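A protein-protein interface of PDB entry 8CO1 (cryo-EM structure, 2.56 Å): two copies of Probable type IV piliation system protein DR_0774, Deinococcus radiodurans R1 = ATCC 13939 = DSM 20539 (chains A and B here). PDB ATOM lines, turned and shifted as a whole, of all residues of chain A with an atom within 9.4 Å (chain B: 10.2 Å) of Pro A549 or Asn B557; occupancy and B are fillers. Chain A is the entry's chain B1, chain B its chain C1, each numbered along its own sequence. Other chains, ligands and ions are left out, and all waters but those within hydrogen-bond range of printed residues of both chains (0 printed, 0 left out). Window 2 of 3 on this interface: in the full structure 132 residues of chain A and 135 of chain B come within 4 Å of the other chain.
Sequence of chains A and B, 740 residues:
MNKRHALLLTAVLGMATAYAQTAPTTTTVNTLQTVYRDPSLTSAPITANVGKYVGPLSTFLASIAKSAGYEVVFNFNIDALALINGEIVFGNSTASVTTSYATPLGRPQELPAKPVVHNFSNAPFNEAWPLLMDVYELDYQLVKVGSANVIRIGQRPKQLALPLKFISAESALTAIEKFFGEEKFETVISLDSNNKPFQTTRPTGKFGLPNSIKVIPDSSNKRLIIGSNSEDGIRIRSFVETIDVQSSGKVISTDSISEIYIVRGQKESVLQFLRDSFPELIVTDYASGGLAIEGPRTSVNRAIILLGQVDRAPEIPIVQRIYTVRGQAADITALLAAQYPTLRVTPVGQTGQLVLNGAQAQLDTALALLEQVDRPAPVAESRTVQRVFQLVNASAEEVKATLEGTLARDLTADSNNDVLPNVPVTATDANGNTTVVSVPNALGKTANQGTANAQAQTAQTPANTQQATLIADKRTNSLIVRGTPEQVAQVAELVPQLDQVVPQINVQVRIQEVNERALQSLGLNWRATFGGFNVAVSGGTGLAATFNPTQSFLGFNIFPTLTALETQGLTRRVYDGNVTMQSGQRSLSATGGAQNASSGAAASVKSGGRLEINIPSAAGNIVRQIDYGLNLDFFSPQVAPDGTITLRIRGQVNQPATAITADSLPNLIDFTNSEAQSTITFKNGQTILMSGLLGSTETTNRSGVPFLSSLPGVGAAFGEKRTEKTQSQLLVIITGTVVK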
ATOM      1  N   GLY A 531     -25.763  14.650 -21.000  1.00  0.00           N
ATOM      2  CA  GLY A 531     -24.801  13.584 -20.776  1.00  0.00           C
ATOM      3  C   GLY A 531     -23.358  13.903 -21.101  1.00  0.00           C
ATOM      4  O   GLY A 531     -22.966  13.952 -22.271  1.00  0.00           O
ATOM      5  N   GLY A 532     -22.547  14.086 -20.061  1.00  0.00           N
ATOM      6  CA  GLY A 532     -21.159  14.448 -20.200  1.00  0.00           C
ATOM      7  C   GLY A 532     -20.899  15.937 -20.323  1.00  0.00           C
ATOM      8  O   GLY A 532     -19.841  16.407 -19.905  1.00  0.00           O
ATOM      9  N   PHE A 533     -21.847  16.688 -20.870  1.00  0.00           N
ATOM     10  CA  PHE A 533     -21.674  18.099 -21.168  1.00  0.00           C
ATOM     11  C   PHE A 533     -22.201  18.979 -20.046  1.00  0.00           C
ATOM     12  O   PHE A 533     -23.121  18.610 -19.316  1.00  0.00           O
ATOM     13  CB  PHE A 533     -22.382  18.461 -22.470  1.00  0.00           C
ATOM     14  CG  PHE A 533     -21.692  17.945 -23.681  1.00  0.00           C
ATOM     15  CD1 PHE A 533     -20.710  18.691 -24.301  1.00  0.00           C
ATOM     16  CD2 PHE A 533     -22.012  16.708 -24.196  1.00  0.00           C
ATOM     17  CE1 PHE A 533     -20.068  18.218 -25.416  1.00  0.00           C
ATOM     18  CE2 PHE A 533     -21.370  16.227 -25.309  1.00  0.00           C
ATOM     19  CZ  PHE A 533     -20.398  16.984 -25.923  1.00  0.00           C
ATOM     20  N   THR A 546     -17.972  22.492 -20.923  1.00  0.00           N
ATOM     21  CA  THR A 546     -16.987  21.480 -20.572  1.00  0.00           C
ATOM     22  C   THR A 546     -17.531  20.106 -20.926  1.00  0.00           C
ATOM     23  O   THR A 546     -18.726  19.930 -21.162  1.00  0.00           O
ATOM     24  CB  THR A 546     -16.614  21.510 -19.085  1.00  0.00           C
ATOM     25  OG1 THR A 546     -17.789  21.323 -18.292  1.00  0.00           O
ATOM     26  CG2 THR A 546     -15.978  22.832 -18.720  1.00  0.00           C
ATOM     27  N   PHE A 547     -16.630  19.132 -20.977  1.00  0.00           N
ATOM     28  CA  PHE A 547     -16.983  17.734 -21.173  1.00  0.00           C
ATOM     29  C   PHE A 547     -16.307  16.892 -20.103  1.00  0.00           C
ATOM     30  O   PHE A 547     -15.158  17.148 -19.736  1.00  0.00           O
ATOM     31  CB  PHE A 547     -16.575  17.237 -22.554  1.00  0.00           C
ATOM     32  CG  PHE A 547     -16.923  15.803 -22.804  1.00  0.00           C
ATOM     33  CD1 PHE A 547     -18.230  15.372 -22.731  1.00  0.00           C
ATOM     34  CD2 PHE A 547     -15.939  14.883 -23.106  1.00  0.00           C
ATOM     35  CE1 PHE A 547     -18.549  14.055 -22.961  1.00  0.00           C
ATOM     36  CE2 PHE A 547     -16.256  13.563 -23.334  1.00  0.00           C
ATOM     37  CZ  PHE A 547     -17.563  13.151 -23.261  1.00  0.00           C
ATOM     38  N   ASN A 548     -17.030  15.901 -19.600  1.00  0.00           N
ATOM     39  CA  ASN A 548     -16.501  14.967 -18.606  1.00  0.00           C
ATOM     40  C   ASN A 548     -16.604  13.553 -19.147  1.00  0.00           C
ATOM     41  O   ASN A 548     -17.721  13.010 -19.240  1.00  0.00           O
ATOM     42  CB  ASN A 548     -17.263  15.091 -17.289  1.00  0.00           C
ATOM     43  CG  ASN A 548     -16.525  14.468 -16.132  1.00  0.00           C
ATOM     44  OD1 ASN A 548     -15.644  13.639 -16.320  1.00  0.00           O
ATOM     45  ND2 ASN A 548     -16.881  14.866 -14.925  1.00  0.00           N
ATOM     46  N   PRO A 549     -15.493  12.911 -19.517  1.00  0.00           N
ATOM     47  CA  PRO A 549     -15.571  11.553 -20.070  1.00  0.00           C
ATOM     48  C   PRO A 549     -15.755  10.465 -19.026  1.00  0.00           C
ATOM     49  O   PRO A 549     -15.951   9.304 -19.403  1.00  0.00           O
ATOM     50  CB  PRO A 549     -14.220  11.392 -20.790  1.00  0.00           C
ATOM     51  CG  PRO A 549     -13.546  12.740 -20.709  1.00  0.00           C
ATOM     52  CD  PRO A 549     -14.114  13.413 -19.519  1.00  0.00           C
ATOM     53  N   THR A 550     -15.704  10.795 -17.738  1.00  0.00           N
ATOM     54  CA  THR A 550     -15.775   9.799 -16.680  1.00  0.00           C
ATOM     55  C   THR A 550     -17.175   9.597 -16.120  1.00  0.00           C
ATOM     56  O   THR A 550     -17.460   8.524 -15.580  1.00  0.00           O
ATOM     57  CB  THR A 550     -14.834  10.180 -15.534  1.00  0.00           C
ATOM     58  OG1 THR A 550     -15.106  11.522 -15.119  1.00  0.00           O
ATOM     59  CG2 THR A 550     -13.390  10.078 -15.975  1.00  0.00           C
ATOM     60  N   GLN A 551     -18.048  10.590 -16.224  1.00  0.00           N
ATOM     61  CA  GLN A 551     -19.409  10.533 -15.710  1.00  0.00           C
ATOM     62  C   GLN A 551     -20.392  10.804 -16.842  1.00  0.00           C
ATOM     63  O   GLN A 551     -20.008  11.001 -17.995  1.00  0.00           O
ATOM     64  CB  GLN A 551     -19.597  11.531 -14.569  1.00  0.00           C
ATOM     65  CG  GLN A 551     -18.798  11.196 -13.331  1.00  0.00           C
ATOM     66  CD  GLN A 551     -18.982  12.207 -12.223  1.00  0.00           C
ATOM     67  OE1 GLN A 551     -19.662  13.215 -12.396  1.00  0.00           O
ATOM     68  NE2 GLN A 551     -18.390  11.933 -11.068  1.00  0.00           N
ATOM     69  N   SER A 552     -21.677  10.815 -16.499  1.00  0.00           N
ATOM     70  CA  SER A 552     -22.722  11.063 -17.488  1.00  0.00           C
ATOM     71  C   SER A 552     -23.991  11.470 -16.760  1.00  0.00           C
ATOM     72  O   SER A 552     -24.485  10.719 -15.917  1.00  0.00           O
ATOM     73  CB  SER A 552     -22.959   9.827 -18.344  1.00  0.00           C
ATOM     74  OG  SER A 552     -23.839  10.107 -19.414  1.00  0.00           O
ATOM     75  N   PHE A 553     -24.511  12.651 -17.080  1.00  0.00           N
ATOM     76  CA  PHE A 553     -25.724  13.145 -16.449  1.00  0.00           C
ATOM     77  C   PHE A 553     -26.938  12.350 -16.915  1.00  0.00           C
ATOM     78  O   PHE A 553     -26.905  11.641 -17.923  1.00  0.00           O
ATOM     79  CB  PHE A 553     -25.940  14.624 -16.769  1.00  0.00           C
ATOM     80  CG  PHE A 553     -24.945  15.544 -16.124  1.00  0.00           C
ATOM     81  CD1 PHE A 553     -24.959  15.756 -14.760  1.00  0.00           C
ATOM     82  CD2 PHE A 553     -24.007  16.211 -16.889  1.00  0.00           C
ATOM     83  CE1 PHE A 553     -24.049  16.607 -14.173  1.00  0.00           C
ATOM     84  CE2 PHE A 553     -23.097  17.061 -16.309  1.00  0.00           C
ATOM     85  CZ  PHE A 553     -23.117  17.260 -14.949  1.00  0.00           C
ATOM     86  N   TRP B 526      -7.796  22.037 -23.058  1.00  0.00           N
ATOM     87  CA  TRP B 526      -8.069  20.630 -22.793  1.00  0.00           C
ATOM     88  C   TRP B 526      -6.887  19.945 -22.115  1.00  0.00           C
ATOM     89  O   TRP B 526      -5.849  20.546 -21.851  1.00  0.00           O
ATOM     90  CB  TRP B 526      -8.443  19.891 -24.075  1.00  0.00           C
ATOM     91  CG  TRP B 526      -7.652  20.238 -25.282  1.00  0.00           C
ATOM     92  CD1 TRP B 526      -7.836  21.306 -26.098  1.00  0.00           C
ATOM     93  CD2 TRP B 526      -6.584  19.478 -25.850  1.00  0.00           C
ATOM     94  NE1 TRP B 526      -6.935  21.275 -27.130  1.00  0.00           N
ATOM     95  CE2 TRP B 526      -6.155  20.157 -27.001  1.00  0.00           C
ATOM     96  CE3 TRP B 526      -5.942  18.290 -25.491  1.00  0.00           C
ATOM     97  CZ2 TRP B 526      -5.115  19.692 -27.794  1.00  0.00           C
ATOM     98  CZ3 TRP B 526      -4.911  17.831 -26.277  1.00  0.00           C
ATOM     99  CH2 TRP B 526      -4.507  18.528 -27.415  1.00  0.00           C
ATOM    100  N   ARG B 527      -7.080  18.658 -21.826  1.00  0.00           N
ATOM    101  CA  ARG B 527      -6.082  17.827 -21.158  1.00  0.00           C
ATOM    102  C   ARG B 527      -6.393  16.373 -21.464  1.00  0.00           C
ATOM    103  O   ARG B 527      -7.465  15.887 -21.099  1.00  0.00           O
ATOM    104  CB  ARG B 527      -6.084  18.067 -19.653  1.00  0.00           C
ATOM    105  CG  ARG B 527      -5.000  17.305 -18.930  1.00  0.00           C
ATOM    106  CD  ARG B 527      -5.091  17.463 -17.426  1.00  0.00           C
ATOM    107  NE  ARG B 527      -6.366  17.001 -16.886  1.00  0.00           N
ATOM    108  CZ  ARG B 527      -6.563  15.797 -16.357  1.00  0.00           C
ATOM    109  NH1 ARG B 527      -5.570  14.923 -16.301  1.00  0.00           N
ATOM    110  NH2 ARG B 527      -7.756  15.467 -15.884  1.00  0.00           N
ATOM    111  N   ALA B 528      -5.467  15.677 -22.114  1.00  0.00           N
ATOM    112  CA  ALA B 528      -5.669  14.298 -22.532  1.00  0.00           C
ATOM    113  C   ALA B 528      -4.716  13.377 -21.786  1.00  0.00           C
ATOM    114  O   ALA B 528      -3.556  13.729 -21.553  1.00  0.00           O
ATOM    115  CB  ALA B 528      -5.464  14.145 -24.036  1.00  0.00           C
ATOM    116  N   THR B 529      -5.206  12.199 -21.403  1.00  0.00           N
ATOM    117  CA  THR B 529      -4.397  11.195 -20.717  1.00  0.00           C
ATOM    118  C   THR B 529      -4.630   9.840 -21.365  1.00  0.00           C
ATOM    119  O   THR B 529      -5.700   9.249 -21.198  1.00  0.00           O
ATOM    120  CB  THR B 529      -4.728  11.119 -19.227  1.00  0.00           C
ATOM    121  OG1 THR B 529      -6.107  10.774 -19.062  1.00  0.00           O
ATOM    122  CG2 THR B 529      -4.453  12.440 -18.539  1.00  0.00           C
ATOM    123  N   PHE B 530      -3.636   9.348 -22.086  1.00  0.00           N
ATOM    124  CA  PHE B 530      -3.589   7.969 -22.548  1.00  0.00           C
ATOM    125  C   PHE B 530      -2.317   7.317 -22.011  1.00  0.00           C
ATOM    126  O   PHE B 530      -1.583   7.910 -21.222  1.00  0.00           O
ATOM    127  CB  PHE B 530      -3.707   7.888 -24.074  1.00  0.00           C
ATOM    128  CG  PHE B 530      -2.773   8.788 -24.819  1.00  0.00           C
ATOM    129  CD1 PHE B 530      -3.028  10.144 -24.920  1.00  0.00           C
ATOM    130  CD2 PHE B 530      -1.662   8.274 -25.458  1.00  0.00           C
ATOM    131  CE1 PHE B 530      -2.180  10.971 -25.610  1.00  0.00           C
ATOM    132  CE2 PHE B 530      -0.810   9.099 -26.157  1.00  0.00           C
ATOM    133  CZ  PHE B 530      -1.071  10.450 -26.233  1.00  0.00           C
ATOM    134  N   GLY B 531      -2.064   6.081 -22.431  1.00  0.00           N
ATOM    135  CA  GLY B 531      -1.121   5.226 -21.730  1.00  0.00           C
ATOM    136  C   GLY B 531       0.280   5.775 -21.568  1.00  0.00           C
ATOM    137  O   GLY B 531       1.066   5.801 -22.518  1.00  0.00           O
ATOM    138  N   PHE B 533       1.199   8.789 -21.246  1.00  0.00           N
ATOM    139  CA  PHE B 533       1.284  10.175 -21.677  1.00  0.00           C
ATOM    140  C   PHE B 533       0.272  11.051 -20.957  1.00  0.00           C
ATOM    141  O   PHE B 533      -0.804  10.600 -20.562  1.00  0.00           O
ATOM    142  CB  PHE B 533       1.065  10.279 -23.183  1.00  0.00           C
ATOM    143  CG  PHE B 533       2.218   9.788 -23.984  1.00  0.00           C
ATOM    144  CD1 PHE B 533       3.245  10.642 -24.334  1.00  0.00           C
ATOM    145  CD2 PHE B 533       2.291   8.468 -24.370  1.00  0.00           C
ATOM    146  CE1 PHE B 533       4.313  10.192 -25.066  1.00  0.00           C
ATOM    147  CE2 PHE B 533       3.360   8.011 -25.101  1.00  0.00           C
ATOM    148  CZ  PHE B 533       4.372   8.875 -25.452  1.00  0.00           C
ATOM    149  N   ASN B 534       0.633  12.320 -20.795  1.00  0.00           N
ATOM    150  CA  ASN B 534      -0.233  13.321 -20.183  1.00  0.00           C
ATOM    151  C   ASN B 534      -0.024  14.627 -20.934  1.00  0.00           C
ATOM    152  O   ASN B 534       0.976  15.313 -20.715  1.00  0.00           O
ATOM    153  CB  ASN B 534       0.080  13.487 -18.700  1.00  0.00           C
ATOM    154  CG  ASN B 534      -1.017  14.187 -17.951  1.00  0.00           C
ATOM    155  OD1 ASN B 534      -1.682  15.071 -18.484  1.00  0.00           O
ATOM    156  ND2 ASN B 534      -1.219  13.798 -16.702  1.00  0.00           N
ATOM    157  N   VAL B 535      -0.965  14.975 -21.803  1.00  0.00           N
ATOM    158  CA  VAL B 535      -0.866  16.151 -22.658  1.00  0.00           C
ATOM    159  C   VAL B 535      -1.852  17.201 -22.170  1.00  0.00           C
ATOM    160  O   VAL B 535      -3.012  16.890 -21.888  1.00  0.00           O
ATOM    161  CB  VAL B 535      -1.135  15.785 -24.127  1.00  0.00           C
ATOM    162  CG1 VAL B 535      -1.041  17.005 -25.000  1.00  0.00           C
ATOM    163  CG2 VAL B 535      -0.159  14.733 -24.580  1.00  0.00           C
ATOM    164  N   ALA B 536      -1.386  18.442 -22.058  1.00  0.00           N
ATOM    165  CA  ALA B 536      -2.223  19.561 -21.640  1.00  0.00           C
ATOM    166  C   ALA B 536      -1.961  20.735 -22.565  1.00  0.00           C
ATOM    167  O   ALA B 536      -0.814  21.162 -22.711  1.00  0.00           O
ATOM    168  CB  ALA B 536      -1.946  19.951 -20.187  1.00  0.00           C
ATOM    169  N   SER B 552       0.516   3.440 -16.261  1.00  0.00           N
ATOM    170  CA  SER B 552      -0.105   3.419 -17.581  1.00  0.00           C
ATOM    171  C   SER B 552      -1.594   3.666 -17.414  1.00  0.00           C
ATOM    172  O   SER B 552      -2.265   2.922 -16.696  1.00  0.00           O
ATOM    173  CB  SER B 552       0.150   2.092 -18.282  1.00  0.00           C
ATOM    174  OG  SER B 552      -0.320   2.121 -19.614  1.00  0.00           O
ATOM    175  N   PHE B 553      -2.106   4.706 -18.065  1.00  0.00           N
ATOM    176  CA  PHE B 553      -3.519   5.034 -17.981  1.00  0.00           C
ATOM    177  C   PHE B 553      -4.360   4.001 -18.724  1.00  0.00           C
ATOM    178  O   PHE B 553      -3.868   3.243 -19.564  1.00  0.00           O
ATOM    179  CB  PHE B 553      -3.790   6.419 -18.568  1.00  0.00           C
ATOM    180  CG  PHE B 553      -3.235   7.551 -17.757  1.00  0.00           C
ATOM    181  CD1 PHE B 553      -3.790   7.886 -16.538  1.00  0.00           C
ATOM    182  CD2 PHE B 553      -2.163   8.290 -18.223  1.00  0.00           C
ATOM    183  CE1 PHE B 553      -3.281   8.930 -15.799  1.00  0.00           C
ATOM    184  CE2 PHE B 553      -1.652   9.334 -17.490  1.00  0.00           C
ATOM    185  CZ  PHE B 553      -2.210   9.655 -16.277  1.00  0.00           C
ATOM    186  N   LEU B 554      -5.651   3.989 -18.411  1.00  0.00           N
ATOM    187  CA  LEU B 554      -6.617   3.127 -19.076  1.00  0.00           C
ATOM    188  C   LEU B 554      -7.382   3.937 -20.114  1.00  0.00           C
ATOM    189  O   LEU B 554      -8.048   4.919 -19.772  1.00  0.00           O
ATOM    190  CB  LEU B 554      -7.584   2.514 -18.068  1.00  0.00           C
ATOM    191  CG  LEU B 554      -7.226   1.167 -17.452  1.00  0.00           C
ATOM    192  CD1 LEU B 554      -8.438   0.609 -16.742  1.00  0.00           C
ATOM    193  CD2 LEU B 554      -6.747   0.206 -18.516  1.00  0.00           C
ATOM    194  N   GLY B 555      -7.287   3.527 -21.370  1.00  0.00           N
ATOM    195  CA  GLY B 555      -8.044   4.171 -22.417  1.00  0.00           C
ATOM    196  C   GLY B 555      -7.604   5.601 -22.675  1.00  0.00           C
ATOM    197  O   GLY B 555      -6.537   6.051 -22.268  1.00  0.00           O
ATOM    198  N   PHE B 556      -8.480   6.322 -23.365  1.00  0.00           N
ATOM    199  CA  PHE B 556      -8.255   7.701 -23.763  1.00  0.00           C
ATOM    200  C   PHE B 556      -9.279   8.610 -23.093  1.00  0.00           C
ATOM    201  O   PHE B 556     -10.475   8.308 -23.083  1.00  0.00           O
ATOM    202  CB  PHE B 556      -8.344   7.834 -25.286  1.00  0.00           C
ATOM    203  CG  PHE B 556      -8.018   9.201 -25.800  1.00  0.00           C
ATOM    204  CD1 PHE B 556      -6.728   9.524 -26.172  1.00  0.00           C
ATOM    205  CD2 PHE B 556      -9.004  10.165 -25.925  1.00  0.00           C
ATOM    206  CE1 PHE B 556      -6.425  10.780 -26.648  1.00  0.00           C
ATOM    207  CE2 PHE B 556      -8.707  11.422 -26.398  1.00  0.00           C
ATOM    208  CZ  PHE B 556      -7.416  11.730 -26.761  1.00  0.00           C
ATOM    209  N   ASN B 557      -8.806   9.718 -22.533  1.00  0.00           N
ATOM    210  CA  ASN B 557      -9.662  10.741 -21.953  1.00  0.00           C
ATOM    211  C   ASN B 557      -9.247  12.091 -22.518  1.00  0.00           C
ATOM    212  O   ASN B 557      -8.076  12.298 -22.835  1.00  0.00           O
ATOM    213  CB  ASN B 557      -9.570  10.745 -20.428  1.00  0.00           C
ATOM    214  CG  ASN B 557     -10.273   9.561 -19.803  1.00  0.00           C
ATOM    215  OD1 ASN B 557     -11.276   9.082 -20.321  1.00  0.00           O
ATOM    216  ND2 ASN B 557      -9.753   9.087 -18.681  1.00  0.00           N
ATOM    217  N   ILE B 558     -10.205  13.009 -22.663  1.00  0.00           N
ATOM    218  CA  ILE B 558      -9.933  14.217 -23.437  1.00  0.00           C
ATOM    219  C   ILE B 558     -10.119  15.511 -22.649  1.00  0.00           C
ATOM    220  O   ILE B 558      -9.419  16.495 -22.908  1.00  0.00           O
ATOM    221  CB  ILE B 558     -10.787  14.222 -24.719  1.00  0.00           C
ATOM    222  CG1 ILE B 558     -10.331  15.326 -25.669  1.00  0.00           C
ATOM    223  CG2 ILE B 558     -12.258  14.345 -24.393  1.00  0.00           C
ATOM    224  CD1 ILE B 558      -8.892  15.224 -26.066  1.00  0.00           C
ATOM    225  N   PHE B 559     -11.035  15.523 -21.681  1.00  0.00           N
ATOM    226  CA  PHE B 559     -11.245  16.619 -20.733  1.00  0.00           C
ATOM    227  C   PHE B 559     -11.167  18.031 -21.337  1.00  0.00           C
ATOM    228  O   PHE B 559     -10.355  18.845 -20.889  1.00  0.00           O
ATOM    229  CB  PHE B 559     -10.273  16.492 -19.565  1.00  0.00           C
ATOM    230  CG  PHE B 559     -10.645  15.440 -18.568  1.00  0.00           C
ATOM    231  CD1 PHE B 559     -11.717  15.621 -17.716  1.00  0.00           C
ATOM    232  CD2 PHE B 559      -9.903  14.279 -18.465  1.00  0.00           C
ATOM    233  CE1 PHE B 559     -12.051  14.655 -16.793  1.00  0.00           C
ATOM    234  CE2 PHE B 559     -10.235  13.313 -17.545  1.00  0.00           C
ATOM    235  CZ  PHE B 559     -11.309  13.501 -16.709  1.00  0.00           C
ATOM    236  N   PRO B 560     -12.008  18.359 -22.317  1.00  0.00           N
ATOM    237  CA  PRO B 560     -11.922  19.681 -22.945  1.00  0.00           C
ATOM    238  C   PRO B 560     -12.715  20.742 -22.187  1.00  0.00           C
ATOM    239  O   PRO B 560     -13.497  20.453 -21.284  1.00  0.00           O
ATOM    240  CB  PRO B 560     -12.502  19.450 -24.342  1.00  0.00           C
ATOM    241  CG  PRO B 560     -13.369  18.270 -24.213  1.00  0.00           C
ATOM    242  CD  PRO B 560     -13.045  17.531 -22.947  1.00  0.00           C
ATOM    243  N   THR B 561     -12.488  21.996 -22.581  1.00  0.00           N
ATOM    244  CA  THR B 561     -13.128  23.153 -21.959  1.00  0.00           C
ATOM    245  C   THR B 561     -13.131  24.305 -22.951  1.00  0.00           C
ATOM    246  O   THR B 561     -12.080  24.658 -23.488  1.00  0.00           O
ATOM    247  CB  THR B 561     -12.400  23.576 -20.680  1.00  0.00           C
ATOM    248  OG1 THR B 561     -12.412  22.499 -19.737  1.00  0.00           O
ATOM    249  CG2 THR B 561     -13.071  24.786 -20.065  1.00  0.00           C
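N of Arg B527 sits close to O of Ile B558 (3.4 Å).
N of Arg B527 sits at hydrogen-bond distance from O of Phe B559, 3.4 Å away.
The backbone carbonyl oxygen (O) of Asn B557 lies within hydrogen-bond range of the backbone NH (N) of Thr B529, 3.2 Å away.
The backbone carbonyl oxygen of Gly A532 is in hydrogen-bond range of the backbone NH of Asn A548.
The side-chain amide oxygen of Asn A548 sits at hydrogen-bond distance from the side-chain hydroxyl of Thr A550 (2.5 Å).
Of the printed residues of chain B, Thr A546 touches Pro B560 (3.7 Å) and Thr B561 (3.7 Å).
Of chain B, only Phe B559 (3.8 Å) comes within 4 Å of Asn A548.
Pro A549 touches just these residues of chain B: Asn B557 (3.8 Å), Ile B558 (3.9 Å) and Phe B559 (3.6 Å).
Trp B526 touches none of the printed residues of chain A.
Phe B530 touches none of the printed residues of chain A.
No residue of chain A comes within 4 Å of Phe B556.
Asn B557 touches just one residue of chain A: Pro A549.
Ile B558 touches two residues of chain A.
Printed residues of chain A within 4 Å of Pro B560: Thr A546 and Phe A547.
Of the printed residues of chain A, Thr B561 touches Thr A546 (3.7 Å).
Along chain A the printed residues that touch a printed residue of chain B span positions 546 to 549.
Among the printed residues, 8 pairs touch across the chains.
Among the printed residues, no Asp or Glu carboxylate lies within 4 Å of a Lys or Arg side-chain nitrogen of the other chain.
Positions printed for both chains: 531, 533, 552 and 553.
Of the 8 pairs that touch across the chains among the printed residues, none has its exchanged pair printed and touching as well.
The backbone NH (N) of Phe A547 sits at hydrogen-bond distance from the backbone carbonyl oxygen (O) of Pro B560.
Thr A546 touches Pro B560.
OG1 of Thr B561 touches CG2 of Thr A546 (3.7 Å).
Ile B558 touches Phe A547.
CE1 of Phe B559 touches OD1 of Asn A548, 3.8 Å away.
OD1 of Asn B557 touches CB of Pro A549, at 3.8 Å.
CG of Pro A549 touches N of Ile B558, at 3.9 Å.
CD of Pro A549 touches CE1 of Phe B559 (3.6 Å).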
